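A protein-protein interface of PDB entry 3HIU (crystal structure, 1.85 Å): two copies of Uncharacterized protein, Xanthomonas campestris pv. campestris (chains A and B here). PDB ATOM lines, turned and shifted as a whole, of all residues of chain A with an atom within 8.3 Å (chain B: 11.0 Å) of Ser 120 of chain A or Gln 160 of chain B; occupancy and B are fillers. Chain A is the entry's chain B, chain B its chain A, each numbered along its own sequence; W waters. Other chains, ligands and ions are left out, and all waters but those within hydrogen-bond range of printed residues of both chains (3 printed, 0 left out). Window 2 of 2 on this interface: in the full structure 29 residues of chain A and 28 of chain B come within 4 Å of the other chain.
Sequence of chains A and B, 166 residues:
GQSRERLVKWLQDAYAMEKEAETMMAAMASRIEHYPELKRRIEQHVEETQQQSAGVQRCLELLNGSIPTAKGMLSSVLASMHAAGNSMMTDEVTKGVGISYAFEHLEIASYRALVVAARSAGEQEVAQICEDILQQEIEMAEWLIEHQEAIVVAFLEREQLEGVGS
The backbone carbonyl oxygen (O) of Met 89 of chain B is in hydrogen-bond range of the guanidinium group (NH1) of Arg 6 of chain A. NH2 of Arg 6 of chain A lies within salt-bridge range of OD1 of Asp 91 of chain B, at 3.1 Å. NE1 of Trp 10 of chain A is in hydrogen-bond range of OD1 of Asp 91 of chain B, at 2.8 Å. The side-chain carboxylate (OE1) of Glu 159 of chain B lies within salt-bridge range of the guanidinium group (NE) of Arg 6 of chain A.
The backbone NH (N) of Phe 155 of chain B sits at hydrogen-bond distance from the side-chain hydroxyl (OH) of Tyr 35 of chain B. The side-chain amide nitrogen (NE2) of Gln 160 of chain B sits at hydrogen-bond distance from the backbone carbonyl oxygen (O) of Leu 156 of chain B, 3.4 Å away.
Gln 2 of chain A touches Glu 159 of chain B (OE1 to OE2, 3.8 Å). Phe 155 of chain B touches Arg 6 of chain A (CE2 to NE, 3.9995 Å). Leu 156 of chain B touches Arg 6 of chain A (CD2 to CG, 3.6 Å). Leu 156 of chain B touches Trp 10 of chain A (CD2 to CH2, 3.9 Å). Ala 113 of chain A touches Val 152 of chain B. Val 116 of chain A touches Val 152 of chain B (CG1 to CG1, 3.7 Å). Val 153 of chain B touches Val 116 of chain A. Leu 156 of chain B touches Val 116 of chain A. CD1 of Leu 156 of chain B touches CA of Ala 117 of chain A (3.8 Å). Ser 120 of chain A touches Gln 160 of chain B.
Ser 120 of chain A touches one residue of chain B. Of chain A, only Ser 120 comes within 4 Å of Gln 160 of chain B. Of chain B, only Glu 159 comes within 4 Å of Gln 2 of chain A. Ser 3 of chain A touches none of the printed residues of chain B. No residue of chain B comes within 4 Å of Ala 118 of chain A. Printed residues of chain A within 4 Å of Glu 159 of chain B: Gln 2 and Arg 6. Printed residues of chain A within 4 Å of Phe 155 of chain B: Arg 6 (3.9995 Å). Printed residues of chain A within 4 Å of Leu 156 of chain B: Arg 6, Trp 10, Val 116 and Ala 117. Printed residues of chain A within 4 Å of Asp 91 of chain B: Arg 6 and Trp 10. Ala 154 of chain B touches none of the printed residues of chain A. Ala 127 of chain A touches none of the printed residues of chain B. The nearest residue of chain A that does not touch Gln 160 of chain B is Gln 2 of chain A (4.3 Å). The nearest printed residue of chain A that does not touch Met 89 of chain B is Gln 2 of chain A (5.8 Å).
Of the 17 printed residues of chain B, 8 touch a printed residue of chain A. Hydrophobic or aromatic side chains of chain A within 4 Å of the printed part of chain B: Trp 10, Ala 113 and Val 116. Among the printed residues, 14 pairs touch across the chains. Among the printed residues, Asp or Glu carboxylates within 4 Å of a Lys or Arg side-chain nitrogen of the other chain: Arg 6 of chain A with Asp 91 of chain B and Arg 6 of chain A with Glu 159 of chain B.
No position is printed for both chains.
Water W3 bridges the guanidinium group of Arg 6 of chain A and the side-chain carboxylate of Asp 91 of chain B. Water W2 lies within hydrogen-bond range of the side-chain amide nitrogen (NE2) of Gln 160 of chain B (2.7 Å), the backbone carbonyl oxygen (O) of Gln 2 of chain A (3.0 Å) and the side-chain carboxylate (OE1) of Glu 159 of chain B (3.2 Å). Water W1 lies within hydrogen-bond range of OE2 of Glu 149 of chain B (3.0 Å) and NH1 of Arg 119 of chain A (3.4 Å).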
ATOM      1  N   GLY A   1       0.738 -19.974   6.120  1.00  0.00           N
ATOM      2  CA  GLY A   1       2.184 -20.095   6.067  1.00  0.00           C
ATOM      3  C   GLY A   1       2.875 -19.142   7.027  1.00  0.00           C
ATOM      4  O   GLY A   1       2.852 -19.347   8.241  1.00  0.00           O
ATOM      5  N   GLN A   2       3.497 -18.096   6.484  1.00  0.00           N
ATOM      6  CA  GLN A   2       4.156 -17.074   7.298  1.00  0.00           C
ATOM      7  C   GLN A   2       3.118 -16.195   7.990  1.00  0.00           C
ATOM      8  O   GLN A   2       3.369 -15.628   9.053  1.00  0.00           O
ATOM      9  CB  GLN A   2       5.089 -16.210   6.440  1.00  0.00           C
ATOM     10  CG  GLN A   2       5.887 -15.178   7.236  1.00  0.00           C
ATOM     11  CD  GLN A   2       6.727 -15.809   8.337  1.00  0.00           C
ATOM     12  OE1 GLN A   2       6.476 -15.597   9.522  1.00  0.00           O
ATOM     13  NE2 GLN A   2       7.720 -16.601   7.946  1.00  0.00           N
ATOM     14  N   SER A   3       1.953 -16.083   7.361  1.00  0.00           N
ATOM     15  CA  SER A   3       0.822 -15.379   7.940  1.00  0.00           C
ATOM     16  C   SER A   3       0.383 -16.054   9.236  1.00  0.00           C
ATOM     17  O   SER A   3       0.285 -15.401  10.269  1.00  0.00           O
ATOM     18  CB  SER A   3      -0.340 -15.321   6.949  1.00  0.00           C
ATOM     19  OG  SER A   3      -0.763 -16.618   6.580  1.00  0.00           O
ATOM     20  N   ARG A   4       0.124 -17.356   9.188  1.00  0.00           N
ATOM     21  CA  ARG A   4      -0.300 -18.058  10.391  1.00  0.00           C
ATOM     22  C   ARG A   4       0.756 -17.980  11.465  1.00  0.00           C
ATOM     23  O   ARG A   4       0.445 -17.755  12.631  1.00  0.00           O
ATOM     24  CB  ARG A   4      -0.592 -19.531  10.125  1.00  0.00           C
ATOM     25  CG  ARG A   4      -0.657 -20.346  11.410  1.00  0.00           C
ATOM     26  CD  ARG A   4      -1.230 -21.734  11.190  1.00  0.00           C
ATOM     27  NE  ARG A   4      -2.621 -21.706  10.739  1.00  0.00           N
ATOM     28  CZ  ARG A   4      -3.385 -22.788  10.623  1.00  0.00           C
ATOM     29  NH1 ARG A   4      -2.892 -23.976  10.937  1.00  0.00           N
ATOM     30  NH2 ARG A   4      -4.638 -22.680  10.203  1.00  0.00           N
ATOM     31  N   ARG A   6       3.162 -15.824  11.945  1.00  0.00           N
ATOM     32  CA  ARG A   6       3.379 -14.510  12.545  1.00  0.00           C
ATOM     33  C   ARG A   6       2.266 -14.215  13.552  1.00  0.00           C
ATOM     34  O   ARG A   6       2.511 -13.686  14.630  1.00  0.00           O
ATOM     35  CB  ARG A   6       3.426 -13.414  11.486  1.00  0.00           C
ATOM     36  CG  ARG A   6       3.261 -12.016  12.068  1.00  0.00           C
ATOM     37  CD  ARG A   6       4.389 -11.708  13.032  1.00  0.00           C
ATOM     38  NE  ARG A   6       5.672 -11.765  12.345  1.00  0.00           N
ATOM     39  CZ  ARG A   6       6.845 -11.897  12.952  1.00  0.00           C
ATOM     40  NH1 ARG A   6       7.959 -11.934  12.231  1.00  0.00           N
ATOM     41  NH2 ARG A   6       6.905 -11.997  14.273  1.00  0.00           N
ATOM     42  N   LEU A   7       1.039 -14.560  13.178  1.00  0.00           N
ATOM     43  CA  LEU A   7      -0.121 -14.469  14.056  1.00  0.00           C
ATOM     44  C   LEU A   7       0.149 -15.294  15.317  1.00  0.00           C
ATOM     45  O   LEU A   7      -0.018 -14.814  16.439  1.00  0.00           O
ATOM     46  CB  LEU A   7      -1.351 -15.023  13.325  1.00  0.00           C
ATOM     47  CG  LEU A   7      -2.763 -14.508  13.616  1.00  0.00           C
ATOM     48  CD1 LEU A   7      -3.781 -15.577  13.281  1.00  0.00           C
ATOM     49  CD2 LEU A   7      -2.908 -14.081  15.056  1.00  0.00           C
ATOM     50  N   TRP A  10       2.821 -13.588  17.559  1.00  0.00           N
ATOM     51  CA  TRP A  10       2.288 -12.498  18.386  1.00  0.00           C
ATOM     52  C   TRP A  10       1.244 -12.985  19.373  1.00  0.00           C
ATOM     53  O   TRP A  10       1.109 -12.433  20.464  1.00  0.00           O
ATOM     54  CB  TRP A  10       1.737 -11.363  17.518  1.00  0.00           C
ATOM     55  CG  TRP A  10       2.827 -10.671  16.785  1.00  0.00           C
ATOM     56  CD1 TRP A  10       4.143 -10.769  17.048  1.00  0.00           C
ATOM     57  CD2 TRP A  10       2.700  -9.762  15.683  1.00  0.00           C
ATOM     58  NE1 TRP A  10       4.862  -9.987  16.178  1.00  0.00           N
ATOM     59  CE2 TRP A  10       3.995  -9.352  15.333  1.00  0.00           C
ATOM     60  CE3 TRP A  10       1.619  -9.254  14.963  1.00  0.00           C
ATOM     61  CZ2 TRP A  10       4.245  -8.464  14.290  1.00  0.00           C
ATOM     62  CZ3 TRP A  10       1.871  -8.365  13.928  1.00  0.00           C
ATOM     63  CH2 TRP A  10       3.170  -7.982  13.603  1.00  0.00           C
ATOM     64  N   ALA A 113      -2.253  -4.569  17.029  1.00  0.00           N
ATOM     65  CA  ALA A 113      -1.397  -5.180  16.013  1.00  0.00           C
ATOM     66  C   ALA A 113      -1.691  -6.670  15.823  1.00  0.00           C
ATOM     67  O   ALA A 113      -1.321  -7.247  14.805  1.00  0.00           O
ATOM     68  CB  ALA A 113       0.070  -4.942  16.319  1.00  0.00           C
ATOM     69  N   LEU A 114      -2.363  -7.289  16.792  1.00  0.00           N
ATOM     70  CA  LEU A 114      -2.863  -8.652  16.614  1.00  0.00           C
ATOM     71  C   LEU A 114      -4.081  -8.712  15.693  1.00  0.00           C
ATOM     72  O   LEU A 114      -4.196  -9.601  14.848  1.00  0.00           O
ATOM     73  CB  LEU A 114      -3.195  -9.307  17.951  1.00  0.00           C
ATOM     74  CG  LEU A 114      -2.204 -10.406  18.317  1.00  0.00           C
ATOM     75  CD1 LEU A 114      -2.270 -10.691  19.806  1.00  0.00           C
ATOM     76  CD2 LEU A 114      -2.505 -11.649  17.502  1.00  0.00           C
ATOM     77  N   VAL A 115      -4.993  -7.767  15.861  1.00  0.00           N
ATOM     78  CA  VAL A 115      -6.135  -7.663  14.968  1.00  0.00           C
ATOM     79  C   VAL A 115      -5.685  -7.524  13.509  1.00  0.00           C
ATOM     80  O   VAL A 115      -6.398  -7.930  12.590  1.00  0.00           O
ATOM     81  CB  VAL A 115      -7.018  -6.472  15.354  1.00  0.00           C
ATOM     82  CG1 VAL A 115      -8.239  -6.404  14.456  1.00  0.00           C
ATOM     83  CG2 VAL A 115      -7.432  -6.584  16.817  1.00  0.00           C
ATOM     84  N   VAL A 116      -4.500  -6.954  13.306  1.00  0.00           N
ATOM     85  CA  VAL A 116      -3.943  -6.777  11.966  1.00  0.00           C
ATOM     86  C   VAL A 116      -3.257  -8.051  11.438  1.00  0.00           C
ATOM     87  O   VAL A 116      -3.385  -8.390  10.258  1.00  0.00           O
ATOM     88  CB  VAL A 116      -2.962  -5.579  11.913  1.00  0.00           C
ATOM     89  CG1 VAL A 116      -2.467  -5.350  10.495  1.00  0.00           C
ATOM     90  CG2 VAL A 116      -3.631  -4.328  12.431  1.00  0.00           C
ATOM     91  N   ALA A 117      -2.533  -8.752  12.310  1.00  0.00           N
ATOM     92  CA  ALA A 117      -1.904 -10.021  11.939  1.00  0.00           C
ATOM     93  C   ALA A 117      -2.947 -11.126  11.767  1.00  0.00           C
ATOM     94  O   ALA A 117      -2.700 -12.126  11.084  1.00  0.00           O
ATOM     95  CB  ALA A 117      -0.850 -10.438  12.969  1.00  0.00           C
ATOM     96  N   ALA A 118      -4.104 -10.949  12.402  1.00  0.00           N
ATOM     97  CA  ALA A 118      -5.219 -11.872  12.226  1.00  0.00           C
ATOM     98  C   ALA A 118      -5.983 -11.569  10.932  1.00  0.00           C
ATOM     99  O   ALA A 118      -6.290 -12.469  10.154  1.00  0.00           O
ATOM    100  CB  ALA A 118      -6.154 -11.813  13.428  1.00  0.00           C
ATOM    101  N   ARG A 119      -6.296 -10.299  10.705  1.00  0.00           N
ATOM    102  CA  ARG A 119      -6.991  -9.926   9.485  1.00  0.00           C
ATOM    103  C   ARG A 119      -6.198 -10.380   8.263  1.00  0.00           C
ATOM    104  O   ARG A 119      -6.713 -11.127   7.416  1.00  0.00           O
ATOM    105  CB  ARG A 119      -7.290  -8.423   9.460  1.00  0.00           C
ATOM    106  CG  ARG A 119      -8.514  -8.075  10.304  1.00  0.00           C
ATOM    107  CD  ARG A 119      -8.828  -6.590  10.364  1.00  0.00           C
ATOM    108  NE  ARG A 119      -9.937  -6.342  11.288  1.00  0.00           N
ATOM    109  CZ  ARG A 119     -10.271  -5.146  11.767  1.00  0.00           C
ATOM    110  NH1 ARG A 119      -9.582  -4.067  11.417  1.00  0.00           N
ATOM    111  NH2 ARG A 119     -11.294  -5.029  12.608  1.00  0.00           N
ATOM    112  N   SER A 120      -4.940  -9.944   8.192  1.00  0.00           N
ATOM    113  CA  SER A 120      -4.029 -10.330   7.111  1.00  0.00           C
ATOM    114  C   SER A 120      -3.974 -11.851   6.896  1.00  0.00           C
ATOM    115  O   SER A 120      -3.821 -12.323   5.768  1.00  0.00           O
ATOM    116  CB  SER A 120      -2.623  -9.759   7.365  1.00  0.00           C
ATOM    117  OG  SER A 120      -1.612 -10.534   6.737  1.00  0.00           O
ATOM    118  N   ALA A 121      -4.099 -12.608   7.985  1.00  0.00           N
ATOM    119  CA  ALA A 121      -4.059 -14.069   7.933  1.00  0.00           C
ATOM    120  C   ALA A 121      -5.427 -14.656   7.584  1.00  0.00           C
ATOM    121  O   ALA A 121      -5.569 -15.873   7.434  1.00  0.00           O
ATOM    122  CB  ALA A 121      -3.555 -14.639   9.253  1.00  0.00           C
ATOM    123  N   GLY A 122      -6.425 -13.785   7.461  1.00  0.00           N
ATOM    124  CA  GLY A 122      -7.775 -14.210   7.153  1.00  0.00           C
ATOM    125  C   GLY A 122      -8.364 -15.082   8.242  1.00  0.00           C
ATOM    126  O   GLY A 122      -9.240 -15.906   7.982  1.00  0.00           O
ATOM    127  N   GLU A 123      -7.862 -14.915   9.461  1.00  0.00           N
ATOM    128  CA  GLU A 123      -8.445 -15.563  10.627  1.00  0.00           C
ATOM    129  C   GLU A 123      -9.348 -14.545  11.292  1.00  0.00           C
ATOM    130  O   GLU A 123      -8.942 -13.852  12.224  1.00  0.00           O
ATOM    131  CB  GLU A 123      -7.360 -16.015  11.613  1.00  0.00           C
ATOM    132  CG  GLU A 123      -6.465 -17.154  11.133  1.00  0.00           C
ATOM    133  CD  GLU A 123      -7.144 -18.519  11.172  1.00  0.00           C
ATOM    134  OE1 GLU A 123      -8.256 -18.630  11.730  1.00  0.00           O
ATOM    135  OE2 GLU A 123      -6.555 -19.486  10.641  1.00  0.00           O
ATOM    136  N   GLN A 124     -10.575 -14.431  10.810  1.00  0.00           N
ATOM    137  CA  GLN A 124     -11.456 -13.389  11.313  1.00  0.00           C
ATOM    138  C   GLN A 124     -11.993 -13.661  12.724  1.00  0.00           C
ATOM    139  O   GLN A 124     -12.316 -12.730  13.450  1.00  0.00           O
ATOM    140  CB  GLN A 124     -12.587 -13.111  10.322  1.00  0.00           C
ATOM    141  CG  GLN A 124     -12.115 -12.510   8.997  1.00  0.00           C
ATOM    142  CD  GLN A 124     -11.603 -11.081   9.135  1.00  0.00           C
ATOM    143  OE1 GLN A 124     -11.897 -10.392  10.114  1.00  0.00           O
ATOM    144  NE2 GLN A 124     -10.836 -10.628   8.143  1.00  0.00           N
ATOM    145  N   ALA A 127      -9.352 -12.541  15.087  1.00  0.00           N
ATOM    146  CA  ALA A 127      -9.384 -11.086  15.086  1.00  0.00           C
ATOM    147  C   ALA A 127     -10.431 -10.521  16.046  1.00  0.00           C
ATOM    148  O   ALA A 127     -10.215  -9.483  16.674  1.00  0.00           O
ATOM    149  CB  ALA A 127      -9.610 -10.570  13.669  1.00  0.00           C
ATOM    150  N   TYR B  35      10.837   3.166   7.750  1.00  0.00           N
ATOM    151  CA  TYR B  35       9.752   4.016   8.227  1.00  0.00           C
ATOM    152  C   TYR B  35      10.219   5.457   8.406  1.00  0.00           C
ATOM    153  O   TYR B  35      10.420   5.921   9.531  1.00  0.00           O
ATOM    154  CB  TYR B  35       9.185   3.441   9.529  1.00  0.00           C
ATOM    155  CG  TYR B  35       8.696   2.030   9.350  1.00  0.00           C
ATOM    156  CD1 TYR B  35       7.455   1.774   8.785  1.00  0.00           C
ATOM    157  CD2 TYR B  35       9.485   0.951   9.711  1.00  0.00           C
ATOM    158  CE1 TYR B  35       7.004   0.479   8.609  1.00  0.00           C
ATOM    159  CE2 TYR B  35       9.047  -0.354   9.529  1.00  0.00           C
ATOM    160  CZ  TYR B  35       7.805  -0.585   8.982  1.00  0.00           C
ATOM    161  OH  TYR B  35       7.363  -1.881   8.797  1.00  0.00           O
ATOM    162  N   MET B  89      12.100 -12.911   9.074  1.00  0.00           N
ATOM    163  CA  MET B  89      12.185 -11.549   9.589  1.00  0.00           C
ATOM    164  C   MET B  89      11.840 -11.531  11.079  1.00  0.00           C
ATOM    165  O   MET B  89      11.188 -12.452  11.581  1.00  0.00           O
ATOM    166  CB  MET B  89      11.248 -10.625   8.804  1.00  0.00           C
ATOM    167  CG  MET B  89      11.598  -9.141   8.885  1.00  0.00           C
ATOM    168  SD  MET B  89      10.430  -8.025   7.778  1.00  0.00           S
ATOM    169  CE  MET B  89      11.186  -6.275   8.184  1.00  0.00           C
ATOM    170  N   THR B  90      12.280 -10.491  11.783  1.00  0.00           N
ATOM    171  CA  THR B  90      12.047 -10.399  13.225  1.00  0.00           C
ATOM    172  C   THR B  90      11.529  -9.029  13.691  1.00  0.00           C
ATOM    173  O   THR B  90      11.638  -8.023  12.986  1.00  0.00           O
ATOM    174  CB  THR B  90      13.279 -10.867  14.040  1.00  0.00           C
ATOM    175  OG1 THR B  90      13.553 -12.236  13.724  1.00  0.00           O
ATOM    176  CG2 THR B  90      13.029 -10.756  15.544  1.00  0.00           C
ATOM    177  N   ASP B  91      11.001  -9.021  14.911  1.00  0.00           N
ATOM    178  CA  ASP B  91      10.003  -8.060  15.361  1.00  0.00           C
ATOM    179  C   ASP B  91      10.402  -6.632  15.725  1.00  0.00           C
ATOM    180  O   ASP B  91       9.533  -5.768  15.761  1.00  0.00           O
ATOM    181  CB  ASP B  91       9.245  -8.664  16.536  1.00  0.00           C
ATOM    182  CG  ASP B  91       7.994  -9.352  16.107  1.00  0.00           C
ATOM    183  OD1 ASP B  91       7.587 -10.326  16.769  1.00  0.00           O
ATOM    184  OD2 ASP B  91       7.416  -8.914  15.094  1.00  0.00           O
ATOM    185  N   GLU B 149      -0.918   1.491  12.916  1.00  0.00           N
ATOM    186  CA  GLU B 149      -1.539   0.524  12.017  1.00  0.00           C
ATOM    187  C   GLU B 149      -0.802   0.354  10.673  1.00  0.00           C
ATOM    188  O   GLU B 149      -0.769  -0.750  10.113  1.00  0.00           O
ATOM    189  CB  GLU B 149      -3.001   0.893  11.795  1.00  0.00           C
ATOM    190  CG  GLU B 149      -3.876  -0.273  11.408  1.00  0.00           C
ATOM    191  CD  GLU B 149      -5.278   0.164  11.045  1.00  0.00           C
ATOM    192  OE1 GLU B 149      -5.455   1.347  10.677  1.00  0.00           O
ATOM    193  OE2 GLU B 149      -6.200  -0.676  11.126  1.00  0.00           O
ATOM    194  N   ALA B 150      -0.209   1.433  10.159  1.00  0.00           N
ATOM    195  CA  ALA B 150       0.529   1.365   8.891  1.00  0.00           C
ATOM    196  C   ALA B 150       1.823   0.568   9.039  1.00  0.00           C
ATOM    197  O   ALA B 150       2.128  -0.303   8.226  1.00  0.00           O
ATOM    198  CB  ALA B 150       0.827   2.778   8.356  1.00  0.00           C
ATOM    199  N   ILE B 151       2.582   0.883  10.085  1.00  0.00           N
ATOM    200  CA  ILE B 151       3.835   0.187  10.367  1.00  0.00           C
ATOM    201  C   ILE B 151       3.624  -1.322  10.458  1.00  0.00           C
ATOM    202  O   ILE B 151       4.364  -2.100   9.847  1.00  0.00           O
ATOM    203  CB  ILE B 151       4.492   0.704  11.659  1.00  0.00           C
ATOM    204  CG1 ILE B 151       4.831   2.195  11.501  1.00  0.00           C
ATOM    205  CG2 ILE B 151       5.723  -0.141  11.987  1.00  0.00           C
ATOM    206  CD1 ILE B 151       5.300   2.891  12.764  1.00  0.00           C
ATOM    207  N   VAL B 152       2.602  -1.729  11.203  1.00  0.00           N
ATOM    208  CA  VAL B 152       2.268  -3.139  11.315  1.00  0.00           C
ATOM    209  C   VAL B 152       1.937  -3.747   9.947  1.00  0.00           C
ATOM    210  O   VAL B 152       2.471  -4.792   9.588  1.00  0.00           O
ATOM    211  CB  VAL B 152       1.099  -3.375  12.283  1.00  0.00           C
ATOM    212  CG1 VAL B 152       0.765  -4.846  12.322  1.00  0.00           C
ATOM    213  CG2 VAL B 152       1.451  -2.873  13.679  1.00  0.00           C
ATOM    214  N   VAL B 153       1.067  -3.078   9.195  1.00  0.00           N
ATOM    215  CA  VAL B 153       0.639  -3.541   7.872  1.00  0.00           C
ATOM    216  C   VAL B 153       1.783  -3.687   6.864  1.00  0.00           C
ATOM    217  O   VAL B 153       1.887  -4.698   6.157  1.00  0.00           O
ATOM    218  CB  VAL B 153      -0.422  -2.594   7.288  1.00  0.00           C
ATOM    219  CG1 VAL B 153      -0.556  -2.780   5.784  1.00  0.00           C
ATOM    220  CG2 VAL B 153      -1.751  -2.813   8.012  1.00  0.00           C
ATOM    221  N   ALA B 154       2.631  -2.665   6.801  1.00  0.00           N
ATOM    222  CA  ALA B 154       3.777  -2.664   5.903  1.00  0.00           C
ATOM    223  C   ALA B 154       4.778  -3.716   6.341  1.00  0.00           C
ATOM    224  O   ALA B 154       5.385  -4.389   5.517  1.00  0.00           O
ATOM    225  CB  ALA B 154       4.426  -1.288   5.869  1.00  0.00           C
ATOM    226  N   PHE B 155       4.955  -3.856   7.645  1.00  0.00           N
ATOM    227  CA  PHE B 155       5.850  -4.879   8.152  1.00  0.00           C
ATOM    228  C   PHE B 155       5.375  -6.256   7.714  1.00  0.00           C
ATOM    229  O   PHE B 155       6.157  -7.063   7.201  1.00  0.00           O
ATOM    230  CB  PHE B 155       5.921  -4.840   9.673  1.00  0.00           C
ATOM    231  CG  PHE B 155       6.740  -5.945  10.249  1.00  0.00           C
ATOM    232  CD1 PHE B 155       8.089  -5.767  10.492  1.00  0.00           C
ATOM    233  CD2 PHE B 155       6.170  -7.178  10.508  1.00  0.00           C
ATOM    234  CE1 PHE B 155       8.851  -6.787  11.006  1.00  0.00           C
ATOM    235  CE2 PHE B 155       6.928  -8.205  11.024  1.00  0.00           C
ATOM    236  CZ  PHE B 155       8.272  -8.008  11.273  1.00  0.00           C
ATOM    237  N   LEU B 156       4.090  -6.519   7.935  1.00  0.00           N
ATOM    238  CA  LEU B 156       3.502  -7.797   7.567  1.00  0.00           C
ATOM    239  C   LEU B 156       3.709  -8.043   6.088  1.00  0.00           C
ATOM    240  O   LEU B 156       4.433  -8.962   5.705  1.00  0.00           O
ATOM    241  CB  LEU B 156       2.010  -7.832   7.902  1.00  0.00           C
ATOM    242  CG  LEU B 156       1.672  -7.955   9.390  1.00  0.00           C
ATOM    243  CD1 LEU B 156       0.164  -7.908   9.615  1.00  0.00           C
ATOM    244  CD2 LEU B 156       2.269  -9.220   9.975  1.00  0.00           C
ATOM    245  N   GLU B 157       3.073  -7.202   5.270  1.00  0.00           N
ATOM    246  CA  GLU B 157       3.131  -7.311   3.813  1.00  0.00           C
ATOM    247  C   GLU B 157       4.549  -7.584   3.349  1.00  0.00           C
ATOM    248  O   GLU B 157       4.802  -8.482   2.549  1.00  0.00           O
ATOM    249  CB  GLU B 157       2.620  -6.020   3.163  1.00  0.00           C
ATOM    250  CG  GLU B 157       1.124  -5.771   3.342  1.00  0.00           C
ATOM    251  CD  GLU B 157       0.647  -4.501   2.650  1.00  0.00           C
ATOM    252  OE1 GLU B 157       1.434  -3.534   2.574  1.00  0.00           O
ATOM    253  OE2 GLU B 157      -0.514  -4.472   2.184  1.00  0.00           O
ATOM    254  N   ARG B 158       5.473  -6.796   3.877  1.00  0.00           N
ATOM    255  CA  ARG B 158       6.874  -6.890   3.519  1.00  0.00           C
ATOM    256  C   ARG B 158       7.439  -8.284   3.809  1.00  0.00           C
ATOM    257  O   ARG B 158       8.135  -8.862   2.979  1.00  0.00           O
ATOM    258  CB  ARG B 158       7.648  -5.807   4.267  1.00  0.00           C
ATOM    259  CG  ARG B 158       9.087  -5.647   3.868  1.00  0.00           C
ATOM    260  CD  ARG B 158       9.749  -4.513   4.653  1.00  0.00           C
ATOM    261  NE  ARG B 158       9.813  -3.261   3.901  1.00  0.00           N
ATOM    262  CZ  ARG B 158       9.228  -2.126   4.264  1.00  0.00           C
ATOM    263  NH1 ARG B 158       8.524  -2.051   5.394  1.00  0.00           N
ATOM    264  NH2 ARG B 158       9.363  -1.052   3.497  1.00  0.00           N
ATOM    265  N   GLU B 159       7.116  -8.840   4.972  1.00  0.00           N
ATOM    266  CA  GLU B 159       7.772 -10.068   5.423  1.00  0.00           C
ATOM    267  C   GLU B 159       7.262 -11.324   4.735  1.00  0.00           C
ATOM    268  O   GLU B 159       7.915 -12.365   4.763  1.00  0.00           O
ATOM    269  CB  GLU B 159       7.671 -10.228   6.943  1.00  0.00           C
ATOM    270  CG  GLU B 159       6.533 -11.121   7.414  1.00  0.00           C
ATOM    271  CD  GLU B 159       6.710 -11.577   8.856  1.00  0.00           C
ATOM    272  OE1 GLU B 159       5.733 -11.497   9.626  1.00  0.00           O
ATOM    273  OE2 GLU B 159       7.826 -12.012   9.219  1.00  0.00           O
ATOM    274  N   GLN B 160       6.095 -11.234   4.115  1.00  0.00           N
ATOM    275  CA  GLN B 160       5.531 -12.398   3.458  1.00  0.00           C
ATOM    276  C   GLN B 160       5.401 -12.162   1.960  1.00  0.00           C
ATOM    277  O   GLN B 160       4.547 -12.746   1.303  1.00  0.00           O
ATOM    278  CB  GLN B 160       4.176 -12.735   4.065  1.00  0.00           C
ATOM    279  CG  GLN B 160       3.092 -11.767   3.676  1.00  0.00           C
ATOM    280  CD  GLN B 160       1.965 -11.745   4.669  1.00  0.00           C
ATOM    281  OE1 GLN B 160       0.793 -11.834   4.300  1.00  0.00           O
ATOM    282  NE2 GLN B 160       2.307 -11.625   5.947  1.00  0.00           N
ATOM    283  N   LEU B 161       6.255 -11.298   1.422  1.00  0.00           N
ATOM    284  CA  LEU B 161       6.222 -10.996   0.002  1.00  0.00           C
ATOM    285  C   LEU B 161       6.253 -12.284  -0.809  1.00  0.00           C
ATOM    286  O   LEU B 161       5.723 -12.347  -1.916  1.00  0.00           O
ATOM    287  CB  LEU B 161       7.400 -10.102  -0.387  1.00  0.00           C
ATOM    288  CG  LEU B 161       7.251  -8.585  -0.279  1.00  0.00           C
ATOM    289  CD1 LEU B 161       8.530  -7.910  -0.741  1.00  0.00           C
ATOM    290  CD2 LEU B 161       6.078  -8.097  -1.113  1.00  0.00           C
HETATM  291  O   HOH W   1      -6.813  -3.193   9.563  1.00  0.00           O
HETATM  292  O   HOH W   2       3.260 -12.828   8.114  1.00  0.00           O
HETATM  293  O   HOH W   3       9.500 -12.027  14.778  1.00  0.00           O
